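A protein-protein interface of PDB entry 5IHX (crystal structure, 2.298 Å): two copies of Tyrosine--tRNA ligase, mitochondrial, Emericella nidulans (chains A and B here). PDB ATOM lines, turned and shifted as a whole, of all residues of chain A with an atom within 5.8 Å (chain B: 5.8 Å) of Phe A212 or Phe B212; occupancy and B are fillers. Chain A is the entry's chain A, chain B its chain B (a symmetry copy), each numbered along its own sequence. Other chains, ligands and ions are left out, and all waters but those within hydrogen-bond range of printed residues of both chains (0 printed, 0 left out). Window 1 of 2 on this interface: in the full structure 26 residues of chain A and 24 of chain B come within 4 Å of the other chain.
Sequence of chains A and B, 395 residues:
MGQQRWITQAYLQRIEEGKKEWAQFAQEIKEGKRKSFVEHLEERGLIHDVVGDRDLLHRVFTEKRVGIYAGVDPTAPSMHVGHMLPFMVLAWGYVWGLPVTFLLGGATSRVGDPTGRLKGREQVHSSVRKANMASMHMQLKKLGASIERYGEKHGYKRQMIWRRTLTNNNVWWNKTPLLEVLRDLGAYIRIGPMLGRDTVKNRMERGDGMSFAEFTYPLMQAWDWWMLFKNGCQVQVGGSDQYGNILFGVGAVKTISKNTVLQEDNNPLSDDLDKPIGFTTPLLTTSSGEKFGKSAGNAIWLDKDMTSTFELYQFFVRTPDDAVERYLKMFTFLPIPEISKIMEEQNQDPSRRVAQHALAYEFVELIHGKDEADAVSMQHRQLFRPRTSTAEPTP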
ATOM      1  N   LEU A 182      -5.034  33.212  11.304  1.00  0.00           N
ATOM      2  CA  LEU A 182      -3.730  33.431  10.690  1.00  0.00           C
ATOM      3  C   LEU A 182      -3.217  34.839  10.977  1.00  0.00           C
ATOM      4  O   LEU A 182      -2.029  35.035  11.225  1.00  0.00           O
ATOM      5  CB  LEU A 182      -3.794  33.193   9.179  1.00  0.00           C
ATOM      6  CG  LEU A 182      -4.124  31.772   8.713  1.00  0.00           C
ATOM      7  CD1 LEU A 182      -4.000  31.665   7.199  1.00  0.00           C
ATOM      8  CD2 LEU A 182      -3.238  30.737   9.393  1.00  0.00           C
ATOM      9  N   GLY A 186      -1.497  32.909  13.734  1.00  0.00           N
ATOM     10  CA  GLY A 186      -0.675  32.142  12.813  1.00  0.00           C
ATOM     11  C   GLY A 186       0.537  32.885  12.278  1.00  0.00           C
ATOM     12  O   GLY A 186       1.585  32.285  12.033  1.00  0.00           O
ATOM     13  N   ALA A 187       0.399  34.194  12.100  1.00  0.00           N
ATOM     14  CA  ALA A 187       1.474  35.006  11.535  1.00  0.00           C
ATOM     15  C   ALA A 187       2.648  35.157  12.499  1.00  0.00           C
ATOM     16  O   ALA A 187       3.756  35.500  12.086  1.00  0.00           O
ATOM     17  CB  ALA A 187       0.940  36.376  11.141  1.00  0.00           C
ATOM     18  N   ILE A 189       3.512  32.696  14.853  1.00  0.00           N
ATOM     19  CA  ILE A 189       3.965  31.385  15.306  1.00  0.00           C
ATOM     20  C   ILE A 189       4.939  30.765  14.317  1.00  0.00           C
ATOM     21  O   ILE A 189       4.622  30.601  13.141  1.00  0.00           O
ATOM     22  CB  ILE A 189       2.773  30.417  15.510  1.00  0.00           C
ATOM     23  CG1 ILE A 189       1.825  30.941  16.590  1.00  0.00           C
ATOM     24  CG2 ILE A 189       3.260  29.016  15.875  1.00  0.00           C
ATOM     25  CD1 ILE A 189       2.459  31.129  17.958  1.00  0.00           C
ATOM     26  N   ARG A 190       6.123  30.413  14.811  1.00  0.00           N
ATOM     27  CA  ARG A 190       7.126  29.739  13.997  1.00  0.00           C
ATOM     28  C   ARG A 190       6.863  28.240  14.009  1.00  0.00           C
ATOM     29  O   ARG A 190       6.599  27.659  15.062  1.00  0.00           O
ATOM     30  CB  ARG A 190       8.534  30.044  14.516  1.00  0.00           C
ATOM     31  CG  ARG A 190       8.908  31.517  14.464  1.00  0.00           C
ATOM     32  CD  ARG A 190       9.150  31.989  13.036  1.00  0.00           C
ATOM     33  NE  ARG A 190       8.899  33.419  12.881  1.00  0.00           N
ATOM     34  N   ILE A 191       6.934  27.614  12.839  1.00  0.00           N
ATOM     35  CA  ILE A 191       6.627  26.193  12.725  1.00  0.00           C
ATOM     36  C   ILE A 191       7.784  25.329  13.220  1.00  0.00           C
ATOM     37  O   ILE A 191       7.589  24.168  13.573  1.00  0.00           O
ATOM     38  CB  ILE A 191       6.285  25.799  11.269  1.00  0.00           C
ATOM     39  CG1 ILE A 191       7.494  25.995  10.346  1.00  0.00           C
ATOM     40  CG2 ILE A 191       5.081  26.598  10.778  1.00  0.00           C
ATOM     41  CD1 ILE A 191       7.287  25.458   8.941  1.00  0.00           C
ATOM     42  N   MET A 194       7.321  24.138  16.748  1.00  0.00           N
ATOM     43  CA  MET A 194       6.185  23.220  16.717  1.00  0.00           C
ATOM     44  C   MET A 194       6.630  21.831  16.275  1.00  0.00           C
ATOM     45  O   MET A 194       6.154  20.821  16.794  1.00  0.00           O
ATOM     46  CB  MET A 194       5.093  23.729  15.773  1.00  0.00           C
ATOM     47  CG  MET A 194       4.329  24.940  16.274  1.00  0.00           C
ATOM     48  SD  MET A 194       3.050  25.472  15.117  1.00  0.00           S
ATOM     49  CE  MET A 194       1.970  24.038  15.096  1.00  0.00           C
ATOM     50  N   MET A 210       1.377  12.412   9.870  1.00  0.00           N
ATOM     51  CA  MET A 210       0.580  13.420  10.565  1.00  0.00           C
ATOM     52  C   MET A 210      -0.059  14.389   9.572  1.00  0.00           C
ATOM     53  O   MET A 210       0.581  14.824   8.613  1.00  0.00           O
ATOM     54  CB  MET A 210       1.456  14.186  11.561  1.00  0.00           C
ATOM     55  CG  MET A 210       0.712  15.200  12.405  1.00  0.00           C
ATOM     56  SD  MET A 210       1.806  16.038  13.567  1.00  0.00           S
ATOM     57  CE  MET A 210       0.612  16.868  14.601  1.00  0.00           C
ATOM     58  N   SER A 211      -1.320  14.733   9.817  1.00  0.00           N
ATOM     59  CA  SER A 211      -2.063  15.631   8.936  1.00  0.00           C
ATOM     60  C   SER A 211      -1.872  17.100   9.309  1.00  0.00           C
ATOM     61  O   SER A 211      -1.390  17.421  10.396  1.00  0.00           O
ATOM     62  CB  SER A 211      -3.552  15.288   8.959  1.00  0.00           C
ATOM     63  OG  SER A 211      -4.166  15.784  10.135  1.00  0.00           O
ATOM     64  N   PHE A 212      -2.260  17.985   8.396  1.00  0.00           N
ATOM     65  CA  PHE A 212      -2.191  19.421   8.637  1.00  0.00           C
ATOM     66  C   PHE A 212      -3.170  19.817   9.733  1.00  0.00           C
ATOM     67  O   PHE A 212      -2.862  20.652  10.583  1.00  0.00           O
ATOM     68  CB  PHE A 212      -2.490  20.200   7.352  1.00  0.00           C
ATOM     69  CG  PHE A 212      -2.321  21.685   7.491  1.00  0.00           C
ATOM     70  CD1 PHE A 212      -1.105  22.288   7.215  1.00  0.00           C
ATOM     71  CD2 PHE A 212      -3.379  22.481   7.901  1.00  0.00           C
ATOM     72  CE1 PHE A 212      -0.948  23.657   7.343  1.00  0.00           C
ATOM     73  CE2 PHE A 212      -3.227  23.849   8.033  1.00  0.00           C
ATOM     74  CZ  PHE A 212      -2.010  24.437   7.752  1.00  0.00           C
ATOM     75  N   ALA A 213      -4.354  19.212   9.703  1.00  0.00           N
ATOM     76  CA  ALA A 213      -5.369  19.443  10.727  1.00  0.00           C
ATOM     77  C   ALA A 213      -4.830  19.151  12.126  1.00  0.00           C
ATOM     78  O   ALA A 213      -4.994  19.959  13.041  1.00  0.00           O
ATOM     79  CB  ALA A 213      -6.598  18.597  10.446  1.00  0.00           C
ATOM     80  N   GLU A 214      -4.188  17.997  12.286  1.00  0.00           N
ATOM     81  CA  GLU A 214      -3.608  17.616  13.572  1.00  0.00           C
ATOM     82  C   GLU A 214      -2.525  18.597  13.996  1.00  0.00           C
ATOM     83  O   GLU A 214      -2.435  18.974  15.165  1.00  0.00           O
ATOM     84  CB  GLU A 214      -3.024  16.202  13.508  1.00  0.00           C
ATOM     85  CG  GLU A 214      -4.061  15.098  13.376  1.00  0.00           C
ATOM     86  CD  GLU A 214      -3.426  13.726  13.234  1.00  0.00           C
ATOM     87  OE1 GLU A 214      -2.700  13.505  12.240  1.00  0.00           O
ATOM     88  OE2 GLU A 214      -3.646  12.871  14.118  1.00  0.00           O
ATOM     89  N   PHE A 215      -1.703  19.000  13.034  1.00  0.00           N
ATOM     90  CA  PHE A 215      -0.621  19.948  13.273  1.00  0.00           C
ATOM     91  C   PHE A 215      -1.169  21.285  13.773  1.00  0.00           C
ATOM     92  O   PHE A 215      -0.492  22.012  14.498  1.00  0.00           O
ATOM     93  CB  PHE A 215       0.190  20.135  11.986  1.00  0.00           C
ATOM     94  CG  PHE A 215       1.466  20.905  12.168  1.00  0.00           C
ATOM     95  CD1 PHE A 215       2.490  20.400  12.951  1.00  0.00           C
ATOM     96  CD2 PHE A 215       1.656  22.118  11.526  1.00  0.00           C
ATOM     97  CE1 PHE A 215       3.672  21.101  13.112  1.00  0.00           C
ATOM     98  CE2 PHE A 215       2.836  22.824  11.679  1.00  0.00           C
ATOM     99  CZ  PHE A 215       3.846  22.314  12.472  1.00  0.00           C
ATOM    100  N   THR A 216      -2.406  21.588  13.390  1.00  0.00           N
ATOM    101  CA  THR A 216      -3.047  22.852  13.742  1.00  0.00           C
ATOM    102  C   THR A 216      -3.726  22.809  15.115  1.00  0.00           C
ATOM    103  O   THR A 216      -4.028  23.851  15.693  1.00  0.00           O
ATOM    104  CB  THR A 216      -4.103  23.241  12.677  1.00  0.00           C
ATOM    105  OG1 THR A 216      -3.520  23.182  11.372  1.00  0.00           O
ATOM    106  CG2 THR A 216      -4.657  24.643  12.918  1.00  0.00           C
ATOM    107  N   TYR A 217      -3.952  21.605  15.636  1.00  0.00           N
ATOM    108  CA  TYR A 217      -4.741  21.432  16.859  1.00  0.00           C
ATOM    109  C   TYR A 217      -4.262  22.321  18.018  1.00  0.00           C
ATOM    110  O   TYR A 217      -5.083  22.950  18.685  1.00  0.00           O
ATOM    111  CB  TYR A 217      -4.745  19.960  17.293  1.00  0.00           C
ATOM    112  CG  TYR A 217      -5.681  19.678  18.450  1.00  0.00           C
ATOM    113  CD1 TYR A 217      -6.961  19.193  18.218  1.00  0.00           C
ATOM    114  CD2 TYR A 217      -5.294  19.904  19.767  1.00  0.00           C
ATOM    115  CE1 TYR A 217      -7.827  18.936  19.259  1.00  0.00           C
ATOM    116  CE2 TYR A 217      -6.156  19.649  20.816  1.00  0.00           C
ATOM    117  CZ  TYR A 217      -7.423  19.165  20.556  1.00  0.00           C
ATOM    118  OH  TYR A 217      -8.290  18.908  21.594  1.00  0.00           O
ATOM    119  N   LEU A 219      -2.995  25.198  17.954  1.00  0.00           N
ATOM    120  CA  LEU A 219      -3.414  26.575  17.716  1.00  0.00           C
ATOM    121  C   LEU A 219      -4.898  26.749  18.031  1.00  0.00           C
ATOM    122  O   LEU A 219      -5.324  27.814  18.480  1.00  0.00           O
ATOM    123  CB  LEU A 219      -3.127  26.993  16.269  1.00  0.00           C
ATOM    124  CG  LEU A 219      -1.679  27.376  15.945  1.00  0.00           C
ATOM    125  CD1 LEU A 219      -0.781  26.150  15.867  1.00  0.00           C
ATOM    126  CD2 LEU A 219      -1.607  28.182  14.651  1.00  0.00           C
ATOM    127  N   LEU B 182     -10.065  22.606   7.422  1.00  0.00           N
ATOM    128  CA  LEU B 182      -9.445  21.448   8.059  1.00  0.00           C
ATOM    129  C   LEU B 182     -10.212  20.169   7.738  1.00  0.00           C
ATOM    130  O   LEU B 182      -9.613  19.118   7.508  1.00  0.00           O
ATOM    131  CB  LEU B 182      -9.361  21.639   9.574  1.00  0.00           C
ATOM    132  CG  LEU B 182      -8.491  22.792  10.085  1.00  0.00           C
ATOM    133  CD1 LEU B 182      -8.376  22.729  11.602  1.00  0.00           C
ATOM    134  CD2 LEU B 182      -7.113  22.806   9.434  1.00  0.00           C
ATOM    135  N   GLY B 186      -7.508  20.037   5.122  1.00  0.00           N
ATOM    136  CA  GLY B 186      -6.441  19.897   6.098  1.00  0.00           C
ATOM    137  C   GLY B 186      -6.282  18.494   6.653  1.00  0.00           C
ATOM    138  O   GLY B 186      -5.171  18.062   6.965  1.00  0.00           O
ATOM    139  N   ALA B 187      -7.395  17.779   6.774  1.00  0.00           N
ATOM    140  CA  ALA B 187      -7.379  16.438   7.345  1.00  0.00           C
ATOM    141  C   ALA B 187      -6.713  15.423   6.418  1.00  0.00           C
ATOM    142  O   ALA B 187      -6.300  14.353   6.863  1.00  0.00           O
ATOM    143  CB  ALA B 187      -8.799  15.991   7.667  1.00  0.00           C
ATOM    144  N   ILE B 189      -4.149  16.264   4.108  1.00  0.00           N
ATOM    145  CA  ILE B 189      -2.817  16.695   3.689  1.00  0.00           C
ATOM    146  C   ILE B 189      -1.800  16.375   4.775  1.00  0.00           C
ATOM    147  O   ILE B 189      -1.943  16.812   5.916  1.00  0.00           O
ATOM    148  CB  ILE B 189      -2.777  18.213   3.379  1.00  0.00           C
ATOM    149  CG1 ILE B 189      -3.742  18.569   2.245  1.00  0.00           C
ATOM    150  CG2 ILE B 189      -1.356  18.661   3.031  1.00  0.00           C
ATOM    151  CD1 ILE B 189      -3.468  17.858   0.931  1.00  0.00           C
ATOM    152  N   ARG B 190      -0.771  15.616   4.409  1.00  0.00           N
ATOM    153  CA  ARG B 190       0.316  15.291   5.325  1.00  0.00           C
ATOM    154  C   ARG B 190       1.373  16.392   5.303  1.00  0.00           C
ATOM    155  O   ARG B 190       1.733  16.894   4.238  1.00  0.00           O
ATOM    156  CB  ARG B 190       0.943  13.943   4.960  1.00  0.00           C
ATOM    157  CG  ARG B 190      -0.028  12.773   5.025  1.00  0.00           C
ATOM    158  N   ILE B 191       1.857  16.775   6.482  1.00  0.00           N
ATOM    159  CA  ILE B 191       2.826  17.864   6.587  1.00  0.00           C
ATOM    160  C   ILE B 191       4.232  17.430   6.186  1.00  0.00           C
ATOM    161  O   ILE B 191       5.067  18.269   5.843  1.00  0.00           O
ATOM    162  CB  ILE B 191       2.866  18.448   8.014  1.00  0.00           C
ATOM    163  CG1 ILE B 191       3.302  17.382   9.029  1.00  0.00           C
ATOM    164  CG2 ILE B 191       1.503  19.009   8.383  1.00  0.00           C
ATOM    165  CD1 ILE B 191       3.541  17.925  10.425  1.00  0.00           C
ATOM    166  N   MET B 194       4.824  18.431   2.674  1.00  0.00           N
ATOM    167  CA  MET B 194       4.833  19.895   2.641  1.00  0.00           C
ATOM    168  C   MET B 194       6.178  20.452   3.083  1.00  0.00           C
ATOM    169  O   MET B 194       6.675  21.430   2.523  1.00  0.00           O
ATOM    170  CB  MET B 194       3.732  20.465   3.535  1.00  0.00           C
ATOM    171  CG  MET B 194       2.322  20.268   3.004  1.00  0.00           C
ATOM    172  SD  MET B 194       1.072  20.986   4.089  1.00  0.00           S
ATOM    173  CE  MET B 194       1.502  22.726   4.006  1.00  0.00           C
ATOM    174  N   MET B 210      10.076  29.870   9.345  1.00  0.00           N
ATOM    175  CA  MET B 210       8.829  30.108   8.623  1.00  0.00           C
ATOM    176  C   MET B 210       7.661  30.183   9.601  1.00  0.00           C
ATOM    177  O   MET B 210       7.622  29.446  10.585  1.00  0.00           O
ATOM    178  CB  MET B 210       8.575  29.002   7.596  1.00  0.00           C
ATOM    179  CG  MET B 210       7.332  29.222   6.744  1.00  0.00           C
ATOM    180  SD  MET B 210       7.034  27.902   5.549  1.00  0.00           S
ATOM    181  CE  MET B 210       8.558  27.912   4.612  1.00  0.00           C
ATOM    182  N   SER B 211       6.711  31.075   9.335  1.00  0.00           N
ATOM    183  CA  SER B 211       5.558  31.230  10.218  1.00  0.00           C
ATOM    184  C   SER B 211       4.487  30.209   9.848  1.00  0.00           C
ATOM    185  O   SER B 211       4.536  29.608   8.774  1.00  0.00           O
ATOM    186  CB  SER B 211       4.986  32.643  10.132  1.00  0.00           C
ATOM    187  OG  SER B 211       4.210  32.797   8.959  1.00  0.00           O
ATOM    188  N   PHE B 212       3.520  30.015  10.739  1.00  0.00           N
ATOM    189  CA  PHE B 212       2.433  29.080  10.477  1.00  0.00           C
ATOM    190  C   PHE B 212       1.567  29.590   9.329  1.00  0.00           C
ATOM    191  O   PHE B 212       1.125  28.815   8.481  1.00  0.00           O
ATOM    192  CB  PHE B 212       1.582  28.869  11.731  1.00  0.00           C
ATOM    193  CG  PHE B 212       0.535  27.804  11.575  1.00  0.00           C
ATOM    194  CD1 PHE B 212       0.827  26.482  11.863  1.00  0.00           C
ATOM    195  CD2 PHE B 212      -0.739  28.122  11.133  1.00  0.00           C
ATOM    196  CE1 PHE B 212      -0.131  25.497  11.717  1.00  0.00           C
ATOM    197  CE2 PHE B 212      -1.700  27.142  10.984  1.00  0.00           C
ATOM    198  CZ  PHE B 212      -1.395  25.827  11.278  1.00  0.00           C
ATOM    199  N   ALA B 213       1.328  30.899   9.315  1.00  0.00           N
ATOM    200  CA  ALA B 213       0.577  31.536   8.240  1.00  0.00           C
ATOM    201  C   ALA B 213       1.202  31.253   6.874  1.00  0.00           C
ATOM    202  O   ALA B 213       0.507  30.878   5.928  1.00  0.00           O
ATOM    203  CB  ALA B 213       0.487  33.031   8.480  1.00  0.00           C
ATOM    204  N   GLU B 214       2.515  31.438   6.775  1.00  0.00           N
ATOM    205  CA  GLU B 214       3.235  31.183   5.529  1.00  0.00           C
ATOM    206  C   GLU B 214       3.127  29.713   5.129  1.00  0.00           C
ATOM    207  O   GLU B 214       2.932  29.388   3.957  1.00  0.00           O
ATOM    208  CB  GLU B 214       4.706  31.585   5.672  1.00  0.00           C
ATOM    209  CG  GLU B 214       4.927  33.086   5.800  1.00  0.00           C
ATOM    210  CD  GLU B 214       6.381  33.444   6.038  1.00  0.00           C
ATOM    211  OE1 GLU B 214       6.937  33.029   7.077  1.00  0.00           O
ATOM    212  OE2 GLU B 214       6.967  34.143   5.183  1.00  0.00           O
ATOM    213  N   PHE B 215       3.256  28.835   6.119  1.00  0.00           N
ATOM    214  CA  PHE B 215       3.152  27.396   5.909  1.00  0.00           C
ATOM    215  C   PHE B 215       1.774  27.008   5.366  1.00  0.00           C
ATOM    216  O   PHE B 215       1.635  26.002   4.672  1.00  0.00           O
ATOM    217  CB  PHE B 215       3.434  26.659   7.225  1.00  0.00           C
ATOM    218  CG  PHE B 215       3.572  25.168   7.077  1.00  0.00           C
ATOM    219  CD1 PHE B 215       4.622  24.623   6.355  1.00  0.00           C
ATOM    220  CD2 PHE B 215       2.666  24.312   7.680  1.00  0.00           C
ATOM    221  CE1 PHE B 215       4.754  23.253   6.225  1.00  0.00           C
ATOM    222  CE2 PHE B 215       2.795  22.942   7.555  1.00  0.00           C
ATOM    223  CZ  PHE B 215       3.838  22.411   6.828  1.00  0.00           C
ATOM    224  N   THR B 216       0.765  27.819   5.679  1.00  0.00           N
ATOM    225  CA  THR B 216      -0.617  27.536   5.291  1.00  0.00           C
ATOM    226  C   THR B 216      -0.950  28.026   3.875  1.00  0.00           C
ATOM    227  O   THR B 216      -1.933  27.586   3.278  1.00  0.00           O
ATOM    228  CB  THR B 216      -1.604  28.183   6.294  1.00  0.00           C
ATOM    229  OG1 THR B 216      -1.248  27.813   7.630  1.00  0.00           O
ATOM    230  CG2 THR B 216      -3.041  27.754   6.022  1.00  0.00           C
ATOM    231  N   TYR B 217      -0.121  28.917   3.338  1.00  0.00           N
ATOM    232  CA  TYR B 217      -0.384  29.549   2.039  1.00  0.00           C
ATOM    233  C   TYR B 217      -0.708  28.551   0.917  1.00  0.00           C
ATOM    234  O   TYR B 217      -1.652  28.774   0.156  1.00  0.00           O
ATOM    235  CB  TYR B 217       0.809  30.427   1.636  1.00  0.00           C
ATOM    236  CG  TYR B 217       0.626  31.170   0.330  1.00  0.00           C
ATOM    237  CD1 TYR B 217      -0.160  32.313   0.257  1.00  0.00           C
ATOM    238  CD2 TYR B 217       1.247  30.728  -0.833  1.00  0.00           C
ATOM    239  CE1 TYR B 217      -0.325  32.991  -0.938  1.00  0.00           C
ATOM    240  CE2 TYR B 217       1.091  31.401  -2.028  1.00  0.00           C
ATOM    241  CZ  TYR B 217       0.303  32.531  -2.077  1.00  0.00           C
ATOM    242  OH  TYR B 217       0.146  33.199  -3.270  1.00  0.00           O
ATOM    243  N   LEU B 219      -2.214  25.744   1.013  1.00  0.00           N
ATOM    244  CA  LEU B 219      -3.571  25.225   1.163  1.00  0.00           C
ATOM    245  C   LEU B 219      -4.612  26.266   0.766  1.00  0.00           C
ATOM    246  O   LEU B 219      -5.675  25.924   0.248  1.00  0.00           O
ATOM    247  CB  LEU B 219      -3.818  24.756   2.600  1.00  0.00           C
ATOM    248  CG  LEU B 219      -3.237  23.382   2.951  1.00  0.00           C
ATOM    249  CD1 LEU B 219      -1.723  23.441   3.110  1.00  0.00           C
ATOM    250  CD2 LEU B 219      -3.888  22.822   4.210  1.00  0.00           C
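Ile A189 touches Ser B211 (O to CA, 3.1 Å).
Arg A190 touches Met B210.
O of Ser B211 touches CG2 of Ile A191, 3.7 Å away.
CD1 of Ile A191 touches CD1 of Phe B215, at 3.8 Å.
Gly B186 touches Ser A211.
CB of Ser A211 touches O of Ala B187, at 3.6 Å.
CZ of Phe A212 touches CZ of Phe B212, 3.8 Å away.
Phe B215 touches Phe A212 (CD2 to CE1, 3.7 Å).
CD2 of Phe A212 touches CD2 of Leu B219 (3.7 Å).
Leu A219 touches Phe B212.
Gly A186 touches Ser B211, and with the chains exchanged Ser A211 touches Gly B186.
Ala A187 touches Ser B211, and with the chains exchanged Ser A211 touches Ala B187.
Ile A189 touches Ser B211, and with the chains exchanged Ser A211 touches Ile B189.
Phe B212 touches its own counterpart, Phe A212.
Positions printed for both chains: 182, 186, 187, 189, 190, 191, 194, 210, 211, 212, 213, 214, 215, 216, 217 and 219.
N of Phe A212 is in hydrogen-bond range of O of Ile B189 (2.8 Å).
O of Gly A186 sits at hydrogen-bond distance from N of Ala B213, at 3.1 Å.
N of Phe A212 lies within hydrogen-bond range of O of Gly B186.
The backbone carbonyl oxygen (O) of Gly B186 is in hydrogen-bond range of the backbone NH (N) of Ala A213, 3.1 Å away.
O of Ile A189 is in hydrogen-bond range of N of Phe B212 (2.7 Å).
O of Gly A186 lies within hydrogen-bond range of N of Phe B212, 3.3 Å away.
N of Ile A191 is in hydrogen-bond range of O of Met B210, at 3.0 Å.
The backbone carbonyl oxygen (O) of Met A210 is in hydrogen-bond range of the backbone NH (N) of Ile B191 (3.2 Å).
Of the printed residues of chain B, Gly A186 touches Ser B211 (3.9 Å), Phe B212 (3.3 Å) and Ala B213 (3.1 Å).
Of the printed residues of chain B, Ile A191 touches Met B210, Ser B211, Phe B212 and Phe B215.
Phe A212 touches seven residues of chain B.
Leu B182 touches none of the printed residues of chain A.
Of the printed residues of chain A, Ala B187 touches Ser A211 and Ala A213.
Of the printed residues of chain A, Phe B212 touches Gly A186, Ile A189, Ile A191, Phe A212, Phe A215, Thr A216 and Leu A219.
Tyr B217 touches none of the printed residues of chain A.
The nearest printed residue of chain A that does not touch Phe B212 is Leu A182 (4.01 Å).
The nearest printed residue of chain B that does not touch Met A210 is Ile B189 (4.2 Å).
The backbone carbonyl oxygen (O) of Leu B182 is in hydrogen-bond range of the backbone NH (N) of Ala B187 (2.7 Å).
N of Ala B213 lies close to OG of Ser B211 (3.5 Å).
The backbone carbonyl oxygen (O) of Phe B212 lies within hydrogen-bond range of the side-chain hydroxyl (OG1) of Thr B216 (2.7 Å).
The side-chain hydroxyl of Ser A211 sits close to the backbone NH of Ala A213, at 3.5 Å.
OE1 of Glu B214 lies within hydrogen-bond range of N of Ser B211, 3.0 Å away.
OG1 of Thr A216 is in hydrogen-bond range of O of Phe A212, at 2.7 Å.
Hydrophobic or aromatic side chains of chain A that line the printed part of chain B: Leu A182, Ile A191, Phe A212, Ala A213, Phe A215 and Leu A219.
Along chain A the printed residues that touch a printed residue of chain B span positions 182 to 219.
Printed residues of chain B that touch a printed residue of chain A: Gly B186, Ala B187, Ile B189, Arg B190, Ile B191, Met B210, Ser B211, Phe B212, Ala B213, Phe B215, Thr B216 and Leu B219.
Hydrophobic or aromatic side chains of chain B within 4 Å of the printed part of chain A: Ile B191, Phe B212, Ala B213, Phe B215 and Leu B219.
Among the printed residues, no Asp or Glu carboxylate lies within 4 Å of a Lys or Arg side-chain nitrogen of the other chain.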
